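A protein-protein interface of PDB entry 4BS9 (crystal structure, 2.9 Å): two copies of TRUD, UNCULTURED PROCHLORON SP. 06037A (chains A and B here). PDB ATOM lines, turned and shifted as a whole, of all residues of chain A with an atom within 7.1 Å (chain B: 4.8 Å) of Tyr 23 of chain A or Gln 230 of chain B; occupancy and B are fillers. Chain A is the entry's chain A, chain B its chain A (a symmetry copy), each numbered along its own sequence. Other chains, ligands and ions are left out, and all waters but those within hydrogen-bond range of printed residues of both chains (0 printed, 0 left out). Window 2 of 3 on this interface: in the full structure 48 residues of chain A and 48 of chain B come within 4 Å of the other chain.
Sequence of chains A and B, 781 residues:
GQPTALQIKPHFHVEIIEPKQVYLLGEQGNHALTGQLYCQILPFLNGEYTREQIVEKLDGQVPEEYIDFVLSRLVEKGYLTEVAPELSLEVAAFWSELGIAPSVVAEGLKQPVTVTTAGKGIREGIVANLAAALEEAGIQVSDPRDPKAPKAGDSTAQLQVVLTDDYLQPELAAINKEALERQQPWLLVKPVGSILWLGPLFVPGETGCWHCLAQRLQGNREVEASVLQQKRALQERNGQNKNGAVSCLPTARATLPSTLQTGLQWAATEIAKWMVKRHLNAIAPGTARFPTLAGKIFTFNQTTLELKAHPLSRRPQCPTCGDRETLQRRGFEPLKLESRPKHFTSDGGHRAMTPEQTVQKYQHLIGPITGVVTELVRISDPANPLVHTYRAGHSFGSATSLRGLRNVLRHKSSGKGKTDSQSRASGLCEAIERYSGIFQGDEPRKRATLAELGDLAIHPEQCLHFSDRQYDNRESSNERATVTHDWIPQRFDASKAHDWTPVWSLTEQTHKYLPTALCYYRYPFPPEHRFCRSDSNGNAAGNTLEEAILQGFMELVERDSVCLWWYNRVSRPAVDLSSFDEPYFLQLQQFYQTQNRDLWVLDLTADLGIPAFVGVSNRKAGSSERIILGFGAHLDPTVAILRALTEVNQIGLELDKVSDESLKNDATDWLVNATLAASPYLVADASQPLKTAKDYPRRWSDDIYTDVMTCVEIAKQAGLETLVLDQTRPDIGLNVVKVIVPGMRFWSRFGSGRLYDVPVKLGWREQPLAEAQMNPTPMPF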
ATOM      1  N   PHE A  12      34.187   7.810 -22.656  1.00  0.00           N
ATOM      2  CA  PHE A  12      32.989   7.600 -23.464  1.00  0.00           C
ATOM      3  C   PHE A  12      32.835   6.130 -23.829  1.00  0.00           C
ATOM      4  O   PHE A  12      33.791   5.485 -24.248  1.00  0.00           O
ATOM      5  CB  PHE A  12      33.042   8.431 -24.746  1.00  0.00           C
ATOM      6  CG  PHE A  12      32.817   9.900 -24.535  1.00  0.00           C
ATOM      7  CD1 PHE A  12      31.700  10.356 -23.851  1.00  0.00           C
ATOM      8  CD2 PHE A  12      33.715  10.828 -25.035  1.00  0.00           C
ATOM      9  CE1 PHE A  12      31.489  11.712 -23.667  1.00  0.00           C
ATOM     10  CE2 PHE A  12      33.506  12.184 -24.860  1.00  0.00           C
ATOM     11  CZ  PHE A  12      32.391  12.629 -24.179  1.00  0.00           C
ATOM     12  N   HIS A  13      31.628   5.602 -23.639  1.00  0.00           N
ATOM     13  CA  HIS A  13      31.240   4.335 -24.244  1.00  0.00           C
ATOM     14  C   HIS A  13      30.642   4.631 -25.619  1.00  0.00           C
ATOM     15  O   HIS A  13      29.574   5.227 -25.738  1.00  0.00           O
ATOM     16  CB  HIS A  13      30.236   3.553 -23.388  1.00  0.00           C
ATOM     17  CG  HIS A  13      29.669   2.358 -24.093  1.00  0.00           C
ATOM     18  ND1 HIS A  13      30.464   1.379 -24.654  1.00  0.00           N
ATOM     19  CD2 HIS A  13      28.391   2.001 -24.365  1.00  0.00           C
ATOM     20  CE1 HIS A  13      29.702   0.466 -25.230  1.00  0.00           C
ATOM     21  NE2 HIS A  13      28.439   0.818 -25.066  1.00  0.00           N
ATOM     22  N   VAL A  14      31.353   4.206 -26.655  1.00  0.00           N
ATOM     23  CA  VAL A  14      30.916   4.399 -28.026  1.00  0.00           C
ATOM     24  C   VAL A  14      29.916   3.324 -28.413  1.00  0.00           C
ATOM     25  O   VAL A  14      30.173   2.135 -28.233  1.00  0.00           O
ATOM     26  CB  VAL A  14      32.112   4.345 -28.983  1.00  0.00           C
ATOM     27  CG1 VAL A  14      31.649   4.378 -30.420  1.00  0.00           C
ATOM     28  CG2 VAL A  14      33.045   5.511 -28.715  1.00  0.00           C
ATOM     29  N   GLU A  15      28.773   3.753 -28.939  1.00  0.00           N
ATOM     30  CA  GLU A  15      27.750   2.848 -29.434  1.00  0.00           C
ATOM     31  C   GLU A  15      27.375   3.290 -30.840  1.00  0.00           C
ATOM     32  O   GLU A  15      26.819   4.374 -31.032  1.00  0.00           O
ATOM     33  CB  GLU A  15      26.536   2.862 -28.509  1.00  0.00           C
ATOM     34  CG  GLU A  15      25.650   1.636 -28.641  1.00  0.00           C
ATOM     35  CD  GLU A  15      26.339   0.341 -28.216  1.00  0.00           C
ATOM     36  OE1 GLU A  15      26.764   0.218 -27.041  1.00  0.00           O
ATOM     37  OE2 GLU A  15      26.446  -0.574 -29.065  1.00  0.00           O
ATOM     38  N   ILE A  16      27.714   2.457 -31.821  1.00  0.00           N
ATOM     39  CA  ILE A  16      27.495   2.774 -33.230  1.00  0.00           C
ATOM     40  C   ILE A  16      26.206   2.124 -33.689  1.00  0.00           C
ATOM     41  O   ILE A  16      26.064   0.910 -33.606  1.00  0.00           O
ATOM     42  CB  ILE A  16      28.659   2.257 -34.100  1.00  0.00           C
ATOM     43  CG1 ILE A  16      29.968   2.950 -33.688  1.00  0.00           C
ATOM     44  CG2 ILE A  16      28.373   2.498 -35.573  1.00  0.00           C
ATOM     45  CD1 ILE A  16      31.215   2.476 -34.420  1.00  0.00           C
ATOM     46  N   ILE A  17      25.273   2.924 -34.185  1.00  0.00           N
ATOM     47  CA  ILE A  17      24.009   2.404 -34.681  1.00  0.00           C
ATOM     48  C   ILE A  17      23.987   2.570 -36.175  1.00  0.00           C
ATOM     49  O   ILE A  17      23.747   3.649 -36.692  1.00  0.00           O
ATOM     50  CB  ILE A  17      22.841   3.093 -33.998  1.00  0.00           C
ATOM     51  CG1 ILE A  17      22.879   2.679 -32.531  1.00  0.00           C
ATOM     52  CG2 ILE A  17      21.522   2.704 -34.658  1.00  0.00           C
ATOM     53  CD1 ILE A  17      21.944   3.450 -31.641  1.00  0.00           C
ATOM     54  N   GLU A  18      24.162   1.441 -36.841  1.00  0.00           N
ATOM     55  CA  GLU A  18      24.957   1.357 -38.053  1.00  0.00           C
ATOM     56  C   GLU A  18      24.820   2.464 -39.079  1.00  0.00           C
ATOM     57  O   GLU A  18      25.765   3.225 -39.250  1.00  0.00           O
ATOM     58  CB  GLU A  18      24.807  -0.005 -38.738  1.00  0.00           C
ATOM     59  CG  GLU A  18      25.746  -0.211 -39.928  1.00  0.00           C
ATOM     60  CD  GLU A  18      27.160   0.347 -39.714  1.00  0.00           C
ATOM     61  OE1 GLU A  18      27.703   0.250 -38.589  1.00  0.00           O
ATOM     62  OE2 GLU A  18      27.738   0.885 -40.684  1.00  0.00           O
ATOM     63  N   GLN A  21      24.366   6.763 -37.315  1.00  0.00           N
ATOM     64  CA  GLN A  21      24.313   7.255 -35.942  1.00  0.00           C
ATOM     65  C   GLN A  21      25.462   6.735 -35.134  1.00  0.00           C
ATOM     66  O   GLN A  21      25.847   5.579 -35.268  1.00  0.00           O
ATOM     67  CB  GLN A  21      23.013   6.795 -35.256  1.00  0.00           C
ATOM     68  CG  GLN A  21      21.870   7.785 -35.344  1.00  0.00           C
ATOM     69  CD  GLN A  21      22.324   9.166 -34.939  1.00  0.00           C
ATOM     70  OE1 GLN A  21      22.995   9.333 -33.922  1.00  0.00           O
ATOM     71  NE2 GLN A  21      22.004  10.157 -35.754  1.00  0.00           N
ATOM     72  N   VAL A  22      25.991   7.596 -34.273  1.00  0.00           N
ATOM     73  CA  VAL A  22      26.961   7.207 -33.258  1.00  0.00           C
ATOM     74  C   VAL A  22      26.677   7.972 -31.977  1.00  0.00           C
ATOM     75  O   VAL A  22      26.416   9.172 -32.003  1.00  0.00           O
ATOM     76  CB  VAL A  22      28.391   7.517 -33.697  1.00  0.00           C
ATOM     77  CG1 VAL A  22      29.350   7.367 -32.530  1.00  0.00           C
ATOM     78  CG2 VAL A  22      28.790   6.596 -34.834  1.00  0.00           C
ATOM     79  N   TYR A  23      26.729   7.270 -30.855  1.00  0.00           N
ATOM     80  CA  TYR A  23      26.458   7.881 -29.580  1.00  0.00           C
ATOM     81  C   TYR A  23      27.697   7.733 -28.723  1.00  0.00           C
ATOM     82  O   TYR A  23      28.282   6.659 -28.666  1.00  0.00           O
ATOM     83  CB  TYR A  23      25.277   7.199 -28.919  1.00  0.00           C
ATOM     84  CG  TYR A  23      23.974   7.372 -29.649  1.00  0.00           C
ATOM     85  CD1 TYR A  23      23.649   6.566 -30.717  1.00  0.00           C
ATOM     86  CD2 TYR A  23      23.054   8.337 -29.262  1.00  0.00           C
ATOM     87  CE1 TYR A  23      22.445   6.716 -31.384  1.00  0.00           C
ATOM     88  CE2 TYR A  23      21.843   8.487 -29.917  1.00  0.00           C
ATOM     89  CZ  TYR A  23      21.545   7.669 -30.974  1.00  0.00           C
ATOM     90  OH  TYR A  23      20.360   7.791 -31.661  1.00  0.00           O
ATOM     91  N   LEU A  24      28.111   8.829 -28.094  1.00  0.00           N
ATOM     92  CA  LEU A  24      29.173   8.815 -27.109  1.00  0.00           C
ATOM     93  C   LEU A  24      28.525   8.967 -25.725  1.00  0.00           C
ATOM     94  O   LEU A  24      27.972  10.027 -25.377  1.00  0.00           O
ATOM     95  CB  LEU A  24      30.193   9.933 -27.390  1.00  0.00           C
ATOM     96  CG  LEU A  24      30.690  10.026 -28.832  1.00  0.00           C
ATOM     97  CD1 LEU A  24      31.857  10.992 -28.949  1.00  0.00           C
ATOM     98  CD2 LEU A  24      31.110   8.663 -29.353  1.00  0.00           C
ATOM     99  N   LEU A  25      28.585   7.899 -24.941  1.00  0.00           N
ATOM    100  CA  LEU A  25      27.889   7.871 -23.669  1.00  0.00           C
ATOM    101  C   LEU A  25      28.887   7.952 -22.529  1.00  0.00           C
ATOM    102  O   LEU A  25      29.773   7.117 -22.410  1.00  0.00           O
ATOM    103  CB  LEU A  25      27.045   6.610 -23.563  1.00  0.00           C
ATOM    104  CG  LEU A  25      26.074   6.433 -24.732  1.00  0.00           C
ATOM    105  CD1 LEU A  25      25.506   5.025 -24.706  1.00  0.00           C
ATOM    106  CD2 LEU A  25      24.961   7.464 -24.681  1.00  0.00           C
ATOM    107  N   ASN A  30      26.452  13.064 -22.411  1.00  0.00           N
ATOM    108  CA  ASN A  30      26.339  12.328 -23.671  1.00  0.00           C
ATOM    109  C   ASN A  30      26.484  13.237 -24.896  1.00  0.00           C
ATOM    110  O   ASN A  30      26.379  14.462 -24.813  1.00  0.00           O
ATOM    111  CB  ASN A  30      24.989  11.633 -23.739  1.00  0.00           C
ATOM    112  CG  ASN A  30      24.788  10.631 -22.613  1.00  0.00           C
ATOM    113  OD1 ASN A  30      25.743   9.989 -22.164  1.00  0.00           O
ATOM    114  ND2 ASN A  30      23.538  10.482 -22.156  1.00  0.00           N
ATOM    115  N   HIS A  31      26.751  12.614 -26.038  1.00  0.00           N
ATOM    116  CA  HIS A  31      26.894  13.320 -27.305  1.00  0.00           C
ATOM    117  C   HIS A  31      26.494  12.390 -28.424  1.00  0.00           C
ATOM    118  O   HIS A  31      26.731  11.186 -28.351  1.00  0.00           O
ATOM    119  CB  HIS A  31      28.340  13.737 -27.529  1.00  0.00           C
ATOM    120  CG  HIS A  31      28.886  14.639 -26.471  1.00  0.00           C
ATOM    121  ND1 HIS A  31      28.836  16.011 -26.564  1.00  0.00           N
ATOM    122  CD2 HIS A  31      29.509  14.363 -25.303  1.00  0.00           C
ATOM    123  CE1 HIS A  31      29.397  16.545 -25.496  1.00  0.00           C
ATOM    124  NE2 HIS A  31      29.812  15.565 -24.713  1.00  0.00           N
ATOM    125  N   ALA A  32      25.887  12.947 -29.461  1.00  0.00           N
ATOM    126  CA  ALA A  32      25.570  12.177 -30.644  1.00  0.00           C
ATOM    127  C   ALA A  32      26.358  12.717 -31.828  1.00  0.00           C
ATOM    128  O   ALA A  32      26.638  13.912 -31.910  1.00  0.00           O
ATOM    129  CB  ALA A  32      24.080  12.222 -30.915  1.00  0.00           C
ATOM    130  N   LEU A  33      26.755  11.819 -32.723  1.00  0.00           N
ATOM    131  CA  LEU A  33      27.343  12.207 -33.992  1.00  0.00           C
ATOM    132  C   LEU A  33      26.518  11.615 -35.100  1.00  0.00           C
ATOM    133  O   LEU A  33      25.958  10.526 -34.958  1.00  0.00           O
ATOM    134  CB  LEU A  33      28.774  11.732 -34.108  1.00  0.00           C
ATOM    135  CG  LEU A  33      29.729  12.445 -33.162  1.00  0.00           C
ATOM    136  CD1 LEU A  33      31.077  11.741 -33.205  1.00  0.00           C
ATOM    137  CD2 LEU A  33      29.866  13.922 -33.499  1.00  0.00           C
ATOM    138  N   LEU A  42      35.023   5.334 -36.606  1.00  0.00           N
ATOM    139  CA  LEU A  42      35.055   5.156 -35.164  1.00  0.00           C
ATOM    140  C   LEU A  42      35.330   3.743 -34.656  1.00  0.00           C
ATOM    141  O   LEU A  42      35.831   3.600 -33.544  1.00  0.00           O
ATOM    142  CB  LEU A  42      33.789   5.707 -34.518  1.00  0.00           C
ATOM    143  CG  LEU A  42      33.994   7.175 -34.119  1.00  0.00           C
ATOM    144  CD1 LEU A  42      34.270   8.070 -35.320  1.00  0.00           C
ATOM    145  CD2 LEU A  42      32.799   7.702 -33.356  1.00  0.00           C
ATOM    146  N   SER B 226      16.735   5.088 -25.118  1.00  0.00           N
ATOM    147  CA  SER B 226      16.596   5.223 -26.580  1.00  0.00           C
ATOM    148  C   SER B 226      17.706   4.537 -27.397  1.00  0.00           C
ATOM    149  O   SER B 226      17.436   3.941 -28.432  1.00  0.00           O
ATOM    150  CB  SER B 226      16.536   6.702 -26.965  1.00  0.00           C
ATOM    151  OG  SER B 226      17.120   6.912 -28.233  1.00  0.00           O
ATOM    152  N   VAL B 227      18.952   4.641 -26.942  1.00  0.00           N
ATOM    153  CA  VAL B 227      20.065   4.002 -27.641  1.00  0.00           C
ATOM    154  C   VAL B 227      19.876   2.492 -27.590  1.00  0.00           C
ATOM    155  O   VAL B 227      20.040   1.798 -28.595  1.00  0.00           O
ATOM    156  CB  VAL B 227      21.437   4.364 -27.028  1.00  0.00           C
ATOM    157  CG1 VAL B 227      22.558   3.629 -27.752  1.00  0.00           C
ATOM    158  CG2 VAL B 227      21.685   5.860 -27.110  1.00  0.00           C
ATOM    159  N   LEU B 228      19.528   2.005 -26.405  1.00  0.00           N
ATOM    160  CA  LEU B 228      19.311   0.582 -26.175  1.00  0.00           C
ATOM    161  C   LEU B 228      18.222   0.028 -27.098  1.00  0.00           C
ATOM    162  O   LEU B 228      18.384  -1.026 -27.720  1.00  0.00           O
ATOM    163  CB  LEU B 228      18.930   0.360 -24.714  1.00  0.00           C
ATOM    164  CG  LEU B 228      18.782  -1.072 -24.207  1.00  0.00           C
ATOM    165  CD1 LEU B 228      20.127  -1.788 -24.189  1.00  0.00           C
ATOM    166  CD2 LEU B 228      18.150  -1.042 -22.818  1.00  0.00           C
ATOM    167  N   GLN B 229      17.116   0.753 -27.189  1.00  0.00           N
ATOM    168  CA  GLN B 229      16.047   0.389 -28.092  1.00  0.00           C
ATOM    169  C   GLN B 229      16.551   0.280 -29.531  1.00  0.00           C
ATOM    170  O   GLN B 229      16.351  -0.738 -30.181  1.00  0.00           O
ATOM    171  CB  GLN B 229      14.953   1.431 -27.992  1.00  0.00           C
ATOM    172  CG  GLN B 229      13.964   1.432 -29.140  1.00  0.00           C
ATOM    173  CD  GLN B 229      12.786   2.338 -28.859  1.00  0.00           C
ATOM    174  OE1 GLN B 229      12.567   2.760 -27.718  1.00  0.00           O
ATOM    175  NE2 GLN B 229      12.016   2.645 -29.896  1.00  0.00           N
ATOM    176  N   GLN B 230      17.207   1.331 -30.016  1.00  0.00           N
ATOM    177  CA  GLN B 230      17.746   1.360 -31.377  1.00  0.00           C
ATOM    178  C   GLN B 230      18.753   0.249 -31.631  1.00  0.00           C
ATOM    179  O   GLN B 230      18.793  -0.312 -32.725  1.00  0.00           O
ATOM    180  CB  GLN B 230      18.418   2.696 -31.669  1.00  0.00           C
ATOM    181  CG  GLN B 230      17.473   3.864 -31.853  1.00  0.00           C
ATOM    182  CD  GLN B 230      18.198   5.189 -31.754  1.00  0.00           C
ATOM    183  OE1 GLN B 230      18.377   5.722 -30.664  1.00  0.00           O
ATOM    184  NE2 GLN B 230      18.628   5.723 -32.888  1.00  0.00           N
ATOM    185  N   LYS B 231      19.570  -0.052 -30.627  1.00  0.00           N
ATOM    186  CA  LYS B 231      20.520  -1.157 -30.716  1.00  0.00           C
ATOM    187  C   LYS B 231      19.811  -2.509 -30.846  1.00  0.00           C
ATOM    188  O   LYS B 231      20.230  -3.350 -31.635  1.00  0.00           O
ATOM    189  CB  LYS B 231      21.442  -1.179 -29.495  1.00  0.00           C
ATOM    190  CG  LYS B 231      22.543  -2.219 -29.590  1.00  0.00           C
ATOM    191  CD  LYS B 231      23.541  -2.021 -28.479  1.00  0.00           C
ATOM    192  CE  LYS B 231      24.683  -3.016 -28.563  1.00  0.00           C
ATOM    193  NZ  LYS B 231      25.586  -2.821 -27.385  1.00  0.00           N
ATOM    194  N   ARG B 232      18.746  -2.714 -30.071  1.00  0.00           N
ATOM    195  CA  ARG B 232      17.991  -3.974 -30.106  1.00  0.00           C
ATOM    196  C   ARG B 232      17.198  -4.175 -31.401  1.00  0.00           C
ATOM    197  O   ARG B 232      17.159  -5.284 -31.930  1.00  0.00           O
ATOM    198  CB  ARG B 232      17.084  -4.095 -28.884  1.00  0.00           C
ATOM    199  CG  ARG B 232      17.895  -4.440 -27.656  1.00  0.00           C
ATOM    200  CD  ARG B 232      17.107  -4.483 -26.364  1.00  0.00           C
ATOM    201  NE  ARG B 232      18.001  -4.930 -25.293  1.00  0.00           N
ATOM    202  CZ  ARG B 232      17.801  -4.745 -23.989  1.00  0.00           C
ATOM    203  NH1 ARG B 232      16.716  -4.107 -23.556  1.00  0.00           N
ATOM    204  NH2 ARG B 232      18.700  -5.199 -23.113  1.00  0.00           N
ATOM    205  N   ALA B 233      16.581  -3.114 -31.917  1.00  0.00           N
ATOM    206  CA  ALA B 233      15.942  -3.161 -33.242  1.00  0.00           C
ATOM    207  C   ALA B 233      16.891  -3.756 -34.286  1.00  0.00           C
ATOM    208  O   ALA B 233      16.545  -4.674 -35.047  1.00  0.00           O
ATOM    209  CB  ALA B 233      15.526  -1.761 -33.668  1.00  0.00           C
ATOM    210  N   LEU B 234      18.106  -3.220 -34.289  1.00  0.00           N
ATOM    211  CA  LEU B 234      19.125  -3.598 -35.252  1.00  0.00           C
ATOM    212  C   LEU B 234      19.554  -5.065 -35.104  1.00  0.00           C
ATOM    213  O   LEU B 234      19.967  -5.685 -36.091  1.00  0.00           O
ATOM    214  CB  LEU B 234      20.346  -2.672 -35.097  1.00  0.00           C
ATOM    215  CG  LEU B 234      20.971  -2.173 -36.400  1.00  0.00           C
ATOM    216  CD1 LEU B 234      20.092  -1.115 -37.059  1.00  0.00           C
ATOM    217  CD2 LEU B 234      22.366  -1.627 -36.132  1.00  0.00           C
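No position is printed for both chains.
Of chain B, only Val 227 (3.6 Å) and Gln 230 (3.0 Å) come within 4 Å of Tyr 23 of chain A. Gln 230 of chain B touches just these residues of chain A: Ile 17 and Tyr 23. Of the printed residues of chain A, Leu 234 of chain B touches Glu 18. Printed residues of chain B within 4 Å of Glu 18 of chain A: Leu 234 (3.6 Å). Of the printed residues of chain B, Glu 15 of chain A touches Val 227 and Lys 231. Of the printed residues of chain A, Val 227 of chain B touches Glu 15 (3.8 Å), Ile 17 (3.9 Å) and Tyr 23 (3.6 Å). Printed residues of chain B within 4 Å of Ile 17 of chain A: Val 227 (3.9 Å) and Gln 230 (3.6 Å). The nearest residue of chain A that does not touch Gln 230 of chain B is Gln 21 of chain A (4.6 Å). The nearest printed residue of chain A that does not touch Lys 231 of chain B is Ile 17 of chain A (4.4 Å).
O of Glu 15 of chain A is in hydrogen-bond range of N of Tyr 23 of chain A, 2.9 Å away. OE1 of Gln 230 of chain B lies within hydrogen-bond range of OG of Ser 226 of chain B, at 3.0 Å. A ring nitrogen (NE2) of His 13 of chain A lies within hydrogen-bond range of the side-chain carboxylate of Glu 15 of chain A (2.7 Å).
Among the printed residues, pairs that only touch across the chains: Glu 15 of chain A with Val 227 of chain B, Ile 17 of chain A with Val 227 of chain B, Ile 17 of chain A with Gln 230 of chain B, Glu 18 of chain A with Leu 234 of chain B and Tyr 23 of chain A with Val 227 of chain B.
The side-chain hydroxyl (OH) of Tyr 23 of chain A lies within hydrogen-bond range of the side-chain amide nitrogen (NE2) of Gln 230 of chain B (3.0 Å). The side-chain carboxylate (OE2) of Glu 15 of chain A is in salt-bridge range of the side-chain amino group (NZ) of Lys 231 of chain B (2.9 Å).
Of the 9 printed residues of chain B, 4 touch a printed residue of chain A. Hydrophobic or aromatic side chains of chain B within 4 Å of the printed part of chain A: Val 227 and Leu 234. Of the 17 printed residues of chain A, 4 touch a printed residue of chain B. Printed residues of chain A that touch a printed residue of chain B: Glu 15, Ile 17, Glu 18 and Tyr 23. Hydrophobic or aromatic side chains of chain A that line the printed part of chain B: Ile 17 and Tyr 23.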
